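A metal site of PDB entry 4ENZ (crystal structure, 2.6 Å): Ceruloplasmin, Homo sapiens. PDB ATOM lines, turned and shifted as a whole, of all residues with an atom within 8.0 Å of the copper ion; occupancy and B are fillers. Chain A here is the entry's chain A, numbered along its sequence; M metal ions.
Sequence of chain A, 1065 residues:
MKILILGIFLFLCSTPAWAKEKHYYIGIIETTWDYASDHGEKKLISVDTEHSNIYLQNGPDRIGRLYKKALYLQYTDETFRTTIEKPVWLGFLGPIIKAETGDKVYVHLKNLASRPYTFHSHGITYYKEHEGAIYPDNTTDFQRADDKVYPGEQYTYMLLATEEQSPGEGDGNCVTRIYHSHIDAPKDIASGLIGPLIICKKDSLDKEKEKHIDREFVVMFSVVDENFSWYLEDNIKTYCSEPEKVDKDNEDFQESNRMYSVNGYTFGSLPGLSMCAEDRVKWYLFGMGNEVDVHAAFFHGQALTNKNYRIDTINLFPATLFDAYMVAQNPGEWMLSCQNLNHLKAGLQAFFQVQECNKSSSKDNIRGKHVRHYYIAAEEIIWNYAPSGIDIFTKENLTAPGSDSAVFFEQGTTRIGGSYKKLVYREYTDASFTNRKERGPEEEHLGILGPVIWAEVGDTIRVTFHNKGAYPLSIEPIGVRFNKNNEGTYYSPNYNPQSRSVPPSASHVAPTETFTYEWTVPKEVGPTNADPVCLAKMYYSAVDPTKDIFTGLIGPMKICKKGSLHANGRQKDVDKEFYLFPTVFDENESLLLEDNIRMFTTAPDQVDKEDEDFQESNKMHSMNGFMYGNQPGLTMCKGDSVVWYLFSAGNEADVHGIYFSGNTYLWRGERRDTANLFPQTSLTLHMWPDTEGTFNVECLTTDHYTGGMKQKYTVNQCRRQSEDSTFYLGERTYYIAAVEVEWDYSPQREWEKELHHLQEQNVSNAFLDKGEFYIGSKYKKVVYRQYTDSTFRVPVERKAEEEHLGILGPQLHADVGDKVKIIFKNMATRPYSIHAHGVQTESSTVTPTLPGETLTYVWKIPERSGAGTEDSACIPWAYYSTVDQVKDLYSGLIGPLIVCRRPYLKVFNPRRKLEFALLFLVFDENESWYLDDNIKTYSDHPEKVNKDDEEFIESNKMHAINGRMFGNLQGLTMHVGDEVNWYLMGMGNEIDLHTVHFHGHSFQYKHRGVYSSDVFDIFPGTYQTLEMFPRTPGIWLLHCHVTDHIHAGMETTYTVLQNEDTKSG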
ATOM      1  N   PHE A 221      21.535  19.306  13.733  1.00  0.00           N
ATOM      2  CA  PHE A 221      21.267  19.972  12.464  1.00  0.00           C
ATOM      3  C   PHE A 221      21.742  19.117  11.291  1.00  0.00           C
ATOM      4  O   PHE A 221      22.921  18.744  11.230  1.00  0.00           O
ATOM      5  CB  PHE A 221      22.009  21.327  12.412  1.00  0.00           C
ATOM      6  CG  PHE A 221      21.274  22.451  13.077  1.00  0.00           C
ATOM      7  CD1 PHE A 221      21.075  22.450  14.433  1.00  0.00           C
ATOM      8  CD2 PHE A 221      20.793  23.511  12.320  1.00  0.00           C
ATOM      9  CE1 PHE A 221      20.374  23.500  15.050  1.00  0.00           C
ATOM     10  CE2 PHE A 221      20.111  24.554  12.913  1.00  0.00           C
ATOM     11  CZ  PHE A 221      19.897  24.557  14.284  1.00  0.00           C
ATOM     12  N   SER A 222      20.859  18.823  10.352  1.00  0.00           N
ATOM     13  CA  SER A 222      21.220  18.034   9.198  1.00  0.00           C
ATOM     14  C   SER A 222      20.229  18.093   8.077  1.00  0.00           C
ATOM     15  O   SER A 222      19.034  18.000   8.305  1.00  0.00           O
ATOM     16  CB  SER A 222      21.360  16.560   9.609  1.00  0.00           C
ATOM     17  OG  SER A 222      21.625  15.732   8.468  1.00  0.00           O
ATOM     18  N   VAL A 223      20.749  18.165   6.856  1.00  0.00           N
ATOM     19  CA  VAL A 223      19.971  17.880   5.654  1.00  0.00           C
ATOM     20  C   VAL A 223      19.855  16.366   5.539  1.00  0.00           C
ATOM     21  O   VAL A 223      20.661  15.727   4.837  1.00  0.00           O
ATOM     22  CB  VAL A 223      20.647  18.486   4.363  1.00  0.00           C
ATOM     23  CG1 VAL A 223      19.837  18.185   3.131  1.00  0.00           C
ATOM     24  CG2 VAL A 223      20.848  20.016   4.516  1.00  0.00           C
ATOM     25  N   TYR A 260      15.543  19.054   5.396  1.00  0.00           N
ATOM     26  CA  TYR A 260      16.339  20.005   6.127  1.00  0.00           C
ATOM     27  C   TYR A 260      15.718  20.129   7.503  1.00  0.00           C
ATOM     28  O   TYR A 260      14.635  20.672   7.635  1.00  0.00           O
ATOM     29  CB  TYR A 260      16.313  21.347   5.411  1.00  0.00           C
ATOM     30  CG  TYR A 260      16.932  21.350   4.027  1.00  0.00           C
ATOM     31  CD1 TYR A 260      16.263  20.843   2.916  1.00  0.00           C
ATOM     32  CD2 TYR A 260      18.171  21.913   3.816  1.00  0.00           C
ATOM     33  CE1 TYR A 260      16.831  20.881   1.647  1.00  0.00           C
ATOM     34  CE2 TYR A 260      18.741  21.958   2.579  1.00  0.00           C
ATOM     35  CZ  TYR A 260      18.077  21.430   1.491  1.00  0.00           C
ATOM     36  OH  TYR A 260      18.683  21.467   0.261  1.00  0.00           O
ATOM     37  N   SER A 261      16.396  19.634   8.518  1.00  0.00           N
ATOM     38  CA  SER A 261      15.720  19.313   9.759  1.00  0.00           C
ATOM     39  C   SER A 261      16.582  19.607  10.968  1.00  0.00           C
ATOM     40  O   SER A 261      17.812  19.642  10.871  1.00  0.00           O
ATOM     41  CB  SER A 261      15.411  17.823   9.765  1.00  0.00           C
ATOM     42  OG  SER A 261      16.649  17.085   9.870  1.00  0.00           O
ATOM     43  N   VAL A 292      26.760  19.693   1.495  1.00  0.00           N
ATOM     44  CA  VAL A 292      25.760  20.739   1.657  1.00  0.00           C
ATOM     45  C   VAL A 292      25.455  21.018   3.107  1.00  0.00           C
ATOM     46  O   VAL A 292      24.745  21.981   3.363  1.00  0.00           O
ATOM     47  CB  VAL A 292      24.409  20.421   0.967  1.00  0.00           C
ATOM     48  CG1 VAL A 292      24.587  20.346  -0.551  1.00  0.00           C
ATOM     49  CG2 VAL A 292      23.806  19.185   1.546  1.00  0.00           C
ATOM     50  N   ASP A 293      25.973  20.225   4.056  1.00  0.00           N
ATOM     51  CA  ASP A 293      25.724  20.489   5.488  1.00  0.00           C
ATOM     52  C   ASP A 293      26.709  21.503   6.084  1.00  0.00           C
ATOM     53  O   ASP A 293      27.511  21.215   7.005  1.00  0.00           O
ATOM     54  CB  ASP A 293      25.678  19.206   6.312  1.00  0.00           C
ATOM     55  CG  ASP A 293      24.507  18.342   5.949  1.00  0.00           C
ATOM     56  OD1 ASP A 293      24.674  17.468   5.065  1.00  0.00           O
ATOM     57  OD2 ASP A 293      23.421  18.544   6.501  1.00  0.00           O
ATOM     58  N   VAL A 294      26.616  22.712   5.559  1.00  0.00           N
ATOM     59  CA  VAL A 294      27.292  23.848   6.118  1.00  0.00           C
ATOM     60  C   VAL A 294      26.237  24.614   6.862  1.00  0.00           C
ATOM     61  O   VAL A 294      25.453  25.372   6.249  1.00  0.00           O
ATOM     62  CB  VAL A 294      27.888  24.684   5.010  1.00  0.00           C
ATOM     63  CG1 VAL A 294      28.226  26.080   5.519  1.00  0.00           C
ATOM     64  CG2 VAL A 294      29.098  23.946   4.432  1.00  0.00           C
ATOM     65  N   HIS A 295      26.171  24.397   8.178  1.00  0.00           N
ATOM     66  CA  HIS A 295      25.112  25.016   8.960  1.00  0.00           C
ATOM     67  C   HIS A 295      25.576  26.205   9.769  1.00  0.00           C
ATOM     68  O   HIS A 295      26.764  26.320  10.074  1.00  0.00           O
ATOM     69  CB  HIS A 295      24.472  24.009   9.902  1.00  0.00           C
ATOM     70  CG  HIS A 295      23.912  22.834   9.199  1.00  0.00           C
ATOM     71  ND1 HIS A 295      22.797  22.921   8.398  1.00  0.00           N
ATOM     72  CD2 HIS A 295      24.352  21.559   9.115  1.00  0.00           C
ATOM     73  CE1 HIS A 295      22.558  21.729   7.867  1.00  0.00           C
ATOM     74  NE2 HIS A 295      23.479  20.880   8.296  1.00  0.00           N
ATOM     75  N   ALA A 296      24.592  27.064  10.121  1.00  0.00           N
ATOM     76  CA  ALA A 296      24.799  28.206  11.031  1.00  0.00           C
ATOM     77  C   ALA A 296      23.667  28.315  12.022  1.00  0.00           C
ATOM     78  O   ALA A 296      22.731  29.065  11.790  1.00  0.00           O
ATOM     79  CB  ALA A 296      24.927  29.480  10.268  1.00  0.00           C
ATOM     80  N   ALA A 297      23.770  27.576  13.117  1.00  0.00           N
ATOM     81  CA  ALA A 297      22.690  27.502  14.113  1.00  0.00           C
ATOM     82  C   ALA A 297      22.496  28.854  14.796  1.00  0.00           C
ATOM     83  O   ALA A 297      23.456  29.451  15.268  1.00  0.00           O
ATOM     84  CB  ALA A 297      22.960  26.413  15.144  1.00  0.00           C
ATOM     85  N   LEU A 316      28.058  24.439  12.270  1.00  0.00           N
ATOM     86  CA  LEU A 316      28.127  23.003  12.452  1.00  0.00           C
ATOM     87  C   LEU A 316      28.338  22.358  11.096  1.00  0.00           C
ATOM     88  O   LEU A 316      27.792  22.826  10.098  1.00  0.00           O
ATOM     89  CB  LEU A 316      26.852  22.478  13.073  1.00  0.00           C
ATOM     90  CG  LEU A 316      26.524  22.933  14.509  1.00  0.00           C
ATOM     91  CD1 LEU A 316      25.033  22.639  14.887  1.00  0.00           C
ATOM     92  CD2 LEU A 316      27.476  22.310  15.528  1.00  0.00           C
ATOM     93  N   SER A 337      17.209  28.818  14.110  1.00  0.00           N
ATOM     94  CA  SER A 337      17.286  28.611  12.677  1.00  0.00           C
ATOM     95  C   SER A 337      18.716  28.476  12.154  1.00  0.00           C
ATOM     96  O   SER A 337      19.680  28.803  12.845  1.00  0.00           O
ATOM     97  CB  SER A 337      16.643  29.775  11.972  1.00  0.00           C
ATOM     98  OG  SER A 337      17.422  30.936  12.191  1.00  0.00           O
ATOM     99  N   CYS A 338      18.813  27.995  10.925  1.00  0.00           N
ATOM    100  CA  CYS A 338      20.067  27.939  10.204  1.00  0.00           C
ATOM    101  C   CYS A 338      20.162  29.141   9.272  1.00  0.00           C
ATOM    102  O   CYS A 338      19.249  29.372   8.470  1.00  0.00           O
ATOM    103  CB  CYS A 338      20.170  26.657   9.363  1.00  0.00           C
ATOM    104  SG  CYS A 338      21.732  26.542   8.537  1.00  0.00           S
ATOM    105  N   GLN A 339      21.271  29.862   9.335  1.00  0.00           N
ATOM    106  CA  GLN A 339      21.391  31.114   8.601  1.00  0.00           C
ATOM    107  C   GLN A 339      22.087  30.928   7.282  1.00  0.00           C
ATOM    108  O   GLN A 339      22.259  31.882   6.543  1.00  0.00           O
ATOM    109  CB  GLN A 339      22.058  32.187   9.460  1.00  0.00           C
ATOM    110  CG  GLN A 339      21.228  32.471  10.719  1.00  0.00           C
ATOM    111  CD  GLN A 339      19.956  33.280  10.443  1.00  0.00           C
ATOM    112  OE1 GLN A 339      20.049  34.450  10.091  1.00  0.00           O
ATOM    113  NE2 GLN A 339      18.788  32.671  10.633  1.00  0.00           N
ATOM    114  N   ASN A 340      22.440  29.673   6.969  1.00  0.00           N
ATOM    115  CA  ASN A 340      22.703  29.268   5.578  1.00  0.00           C
ATOM    116  C   ASN A 340      21.427  29.575   4.840  1.00  0.00           C
ATOM    117  O   ASN A 340      20.394  28.986   5.089  1.00  0.00           O
ATOM    118  CB  ASN A 340      23.009  27.759   5.482  1.00  0.00           C
ATOM    119  CG  ASN A 340      23.271  27.298   4.056  1.00  0.00           C
ATOM    120  OD1 ASN A 340      22.743  27.855   3.098  1.00  0.00           O
ATOM    121  ND2 ASN A 340      24.085  26.250   3.924  1.00  0.00           N
ATOM    122  N   LEU A 341      21.508  30.515   3.921  1.00  0.00           N
ATOM    123  CA  LEU A 341      20.306  31.033   3.320  1.00  0.00           C
ATOM    124  C   LEU A 341      19.594  29.990   2.500  1.00  0.00           C
ATOM    125  O   LEU A 341      18.364  29.931   2.491  1.00  0.00           O
ATOM    126  CB  LEU A 341      20.639  32.277   2.502  1.00  0.00           C
ATOM    127  CG  LEU A 341      21.263  33.399   3.346  1.00  0.00           C
ATOM    128  CD1 LEU A 341      21.641  34.557   2.454  1.00  0.00           C
ATOM    129  CD2 LEU A 341      20.328  33.880   4.445  1.00  0.00           C
ATOM    130  N   ASN A 342      20.335  29.129   1.808  1.00  0.00           N
ATOM    131  CA  ASN A 342      19.694  27.996   1.124  1.00  0.00           C
ATOM    132  C   ASN A 342      18.923  27.076   2.068  1.00  0.00           C
ATOM    133  O   ASN A 342      17.816  26.642   1.723  1.00  0.00           O
ATOM    134  CB  ASN A 342      20.676  27.215   0.274  1.00  0.00           C
ATOM    135  CG  ASN A 342      20.964  27.906  -1.024  1.00  0.00           C
ATOM    136  OD1 ASN A 342      20.219  28.803  -1.437  1.00  0.00           O
ATOM    137  ND2 ASN A 342      22.053  27.509  -1.690  1.00  0.00           N
ATOM    138  N   HIS A 343      19.475  26.861   3.274  1.00  0.00           N
ATOM    139  CA  HIS A 343      18.799  26.074   4.329  1.00  0.00           C
ATOM    140  C   HIS A 343      17.604  26.794   4.932  1.00  0.00           C
ATOM    141  O   HIS A 343      16.534  26.214   5.069  1.00  0.00           O
ATOM    142  CB  HIS A 343      19.778  25.708   5.447  1.00  0.00           C
ATOM    143  CG  HIS A 343      20.879  24.777   5.022  1.00  0.00           C
ATOM    144  ND1 HIS A 343      21.802  24.273   5.909  1.00  0.00           N
ATOM    145  CD2 HIS A 343      21.187  24.247   3.806  1.00  0.00           C
ATOM    146  CE1 HIS A 343      22.650  23.498   5.258  1.00  0.00           C
ATOM    147  NE2 HIS A 343      22.296  23.467   3.982  1.00  0.00           N
ATOM    148  N   LEU A 344      17.777  28.063   5.277  1.00  0.00           N
ATOM    149  CA  LEU A 344      16.701  28.835   5.895  1.00  0.00           C
ATOM    150  C   LEU A 344      15.448  28.717   5.033  1.00  0.00           C
ATOM    151  O   LEU A 344      14.336  28.521   5.535  1.00  0.00           O
ATOM    152  CB  LEU A 344      17.120  30.304   6.058  1.00  0.00           C
ATOM    153  CG  LEU A 344      16.245  31.276   6.881  1.00  0.00           C
ATOM    154  CD1 LEU A 344      16.193  30.909   8.370  1.00  0.00           C
ATOM    155  CD2 LEU A 344      16.749  32.701   6.680  1.00  0.00           C
ATOM    156  N   LEU A 348      14.906  25.121   7.524  1.00  0.00           N
ATOM    157  CA  LEU A 348      15.662  24.614   8.680  1.00  0.00           C
ATOM    158  C   LEU A 348      15.436  25.533   9.915  1.00  0.00           C
ATOM    159  O   LEU A 348      16.260  26.399  10.265  1.00  0.00           O
ATOM    160  CB  LEU A 348      17.149  24.395   8.355  1.00  0.00           C
ATOM    161  CG  LEU A 348      17.809  23.236   9.122  1.00  0.00           C
ATOM    162  CD1 LEU A 348      19.286  22.983   8.702  1.00  0.00           C
ATOM    163  CD2 LEU A 348      17.735  23.481  10.622  1.00  0.00           C
ATOM    164  N   GLU A 652      26.054  27.466   1.451  1.00  0.00           N
ATOM    165  CA  GLU A 652      27.142  26.471   1.453  1.00  0.00           C
ATOM    166  C   GLU A 652      28.374  26.840   0.626  1.00  0.00           C
ATOM    167  O   GLU A 652      29.482  26.400   0.958  1.00  0.00           O
ATOM    168  CB  GLU A 652      26.639  25.072   1.041  1.00  0.00           C
ATOM    169  CG  GLU A 652      25.906  24.995  -0.312  1.00  0.00           C
ATOM    170  CD  GLU A 652      24.402  25.165  -0.169  1.00  0.00           C
ATOM    171  OE1 GLU A 652      23.962  25.629   0.905  1.00  0.00           O
ATOM    172  OE2 GLU A 652      23.667  24.846  -1.119  1.00  0.00           O
ATOM    173  N   PRO A 679      28.551  31.155   6.776  1.00  0.00           N
ATOM    174  CA  PRO A 679      27.425  32.043   6.930  1.00  0.00           C
ATOM    175  C   PRO A 679      27.263  32.511   8.346  1.00  0.00           C
ATOM    176  O   PRO A 679      27.244  31.714   9.289  1.00  0.00           O
ATOM    177  CB  PRO A 679      26.248  31.169   6.510  1.00  0.00           C
ATOM    178  CG  PRO A 679      26.867  30.301   5.436  1.00  0.00           C
ATOM    179  CD  PRO A 679      28.191  29.937   6.020  1.00  0.00           C
HETATM  180 CU    CU M   1      21.944  24.550   7.818  1.00  0.00          CU
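A ring nitrogen (NE2) of His 295 lies within hydrogen-bond range of the side-chain carboxylate (OD2) of Asp 293. The backbone NH (N) of His 295 sits at hydrogen-bond distance from the backbone carbonyl oxygen (O) of Leu 316 (3.0 Å). A ring nitrogen (NE2) of His 343 sits at hydrogen-bond distance from the side-chain amide nitrogen (ND2) of Asn 340 (3.3 Å). O of Val 292 lies within hydrogen-bond range of NE2 of His 343 (2.9 Å). The backbone carbonyl oxygen (O) of Leu 348 lies within hydrogen-bond range of the backbone NH (N) of Cys 338 (3.1 Å). SG of Cys 338 lies close to N of Asn 340 (3.6 Å). The side-chain sulfur of Cys 338 sits close to the backbone NH of Ala 296, at 3.3 Å. The side-chain amide nitrogen of Asn 340 sits at hydrogen-bond distance from the backbone carbonyl oxygen of Val 294, at 2.8 Å.
Merely in contact with the copper ion: Val 294 and Leu 348. Five residues have an atom within 4 Å of the copper ion: Val 294, His 295, Cys 338, His 343 and Leu 348. Along chain A the residues within 4 Å of the copper ion span positions 294 to 348.
The copper ion is bound by ND1 of His 295, ND1 of His 343 and SG of Cys 338.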
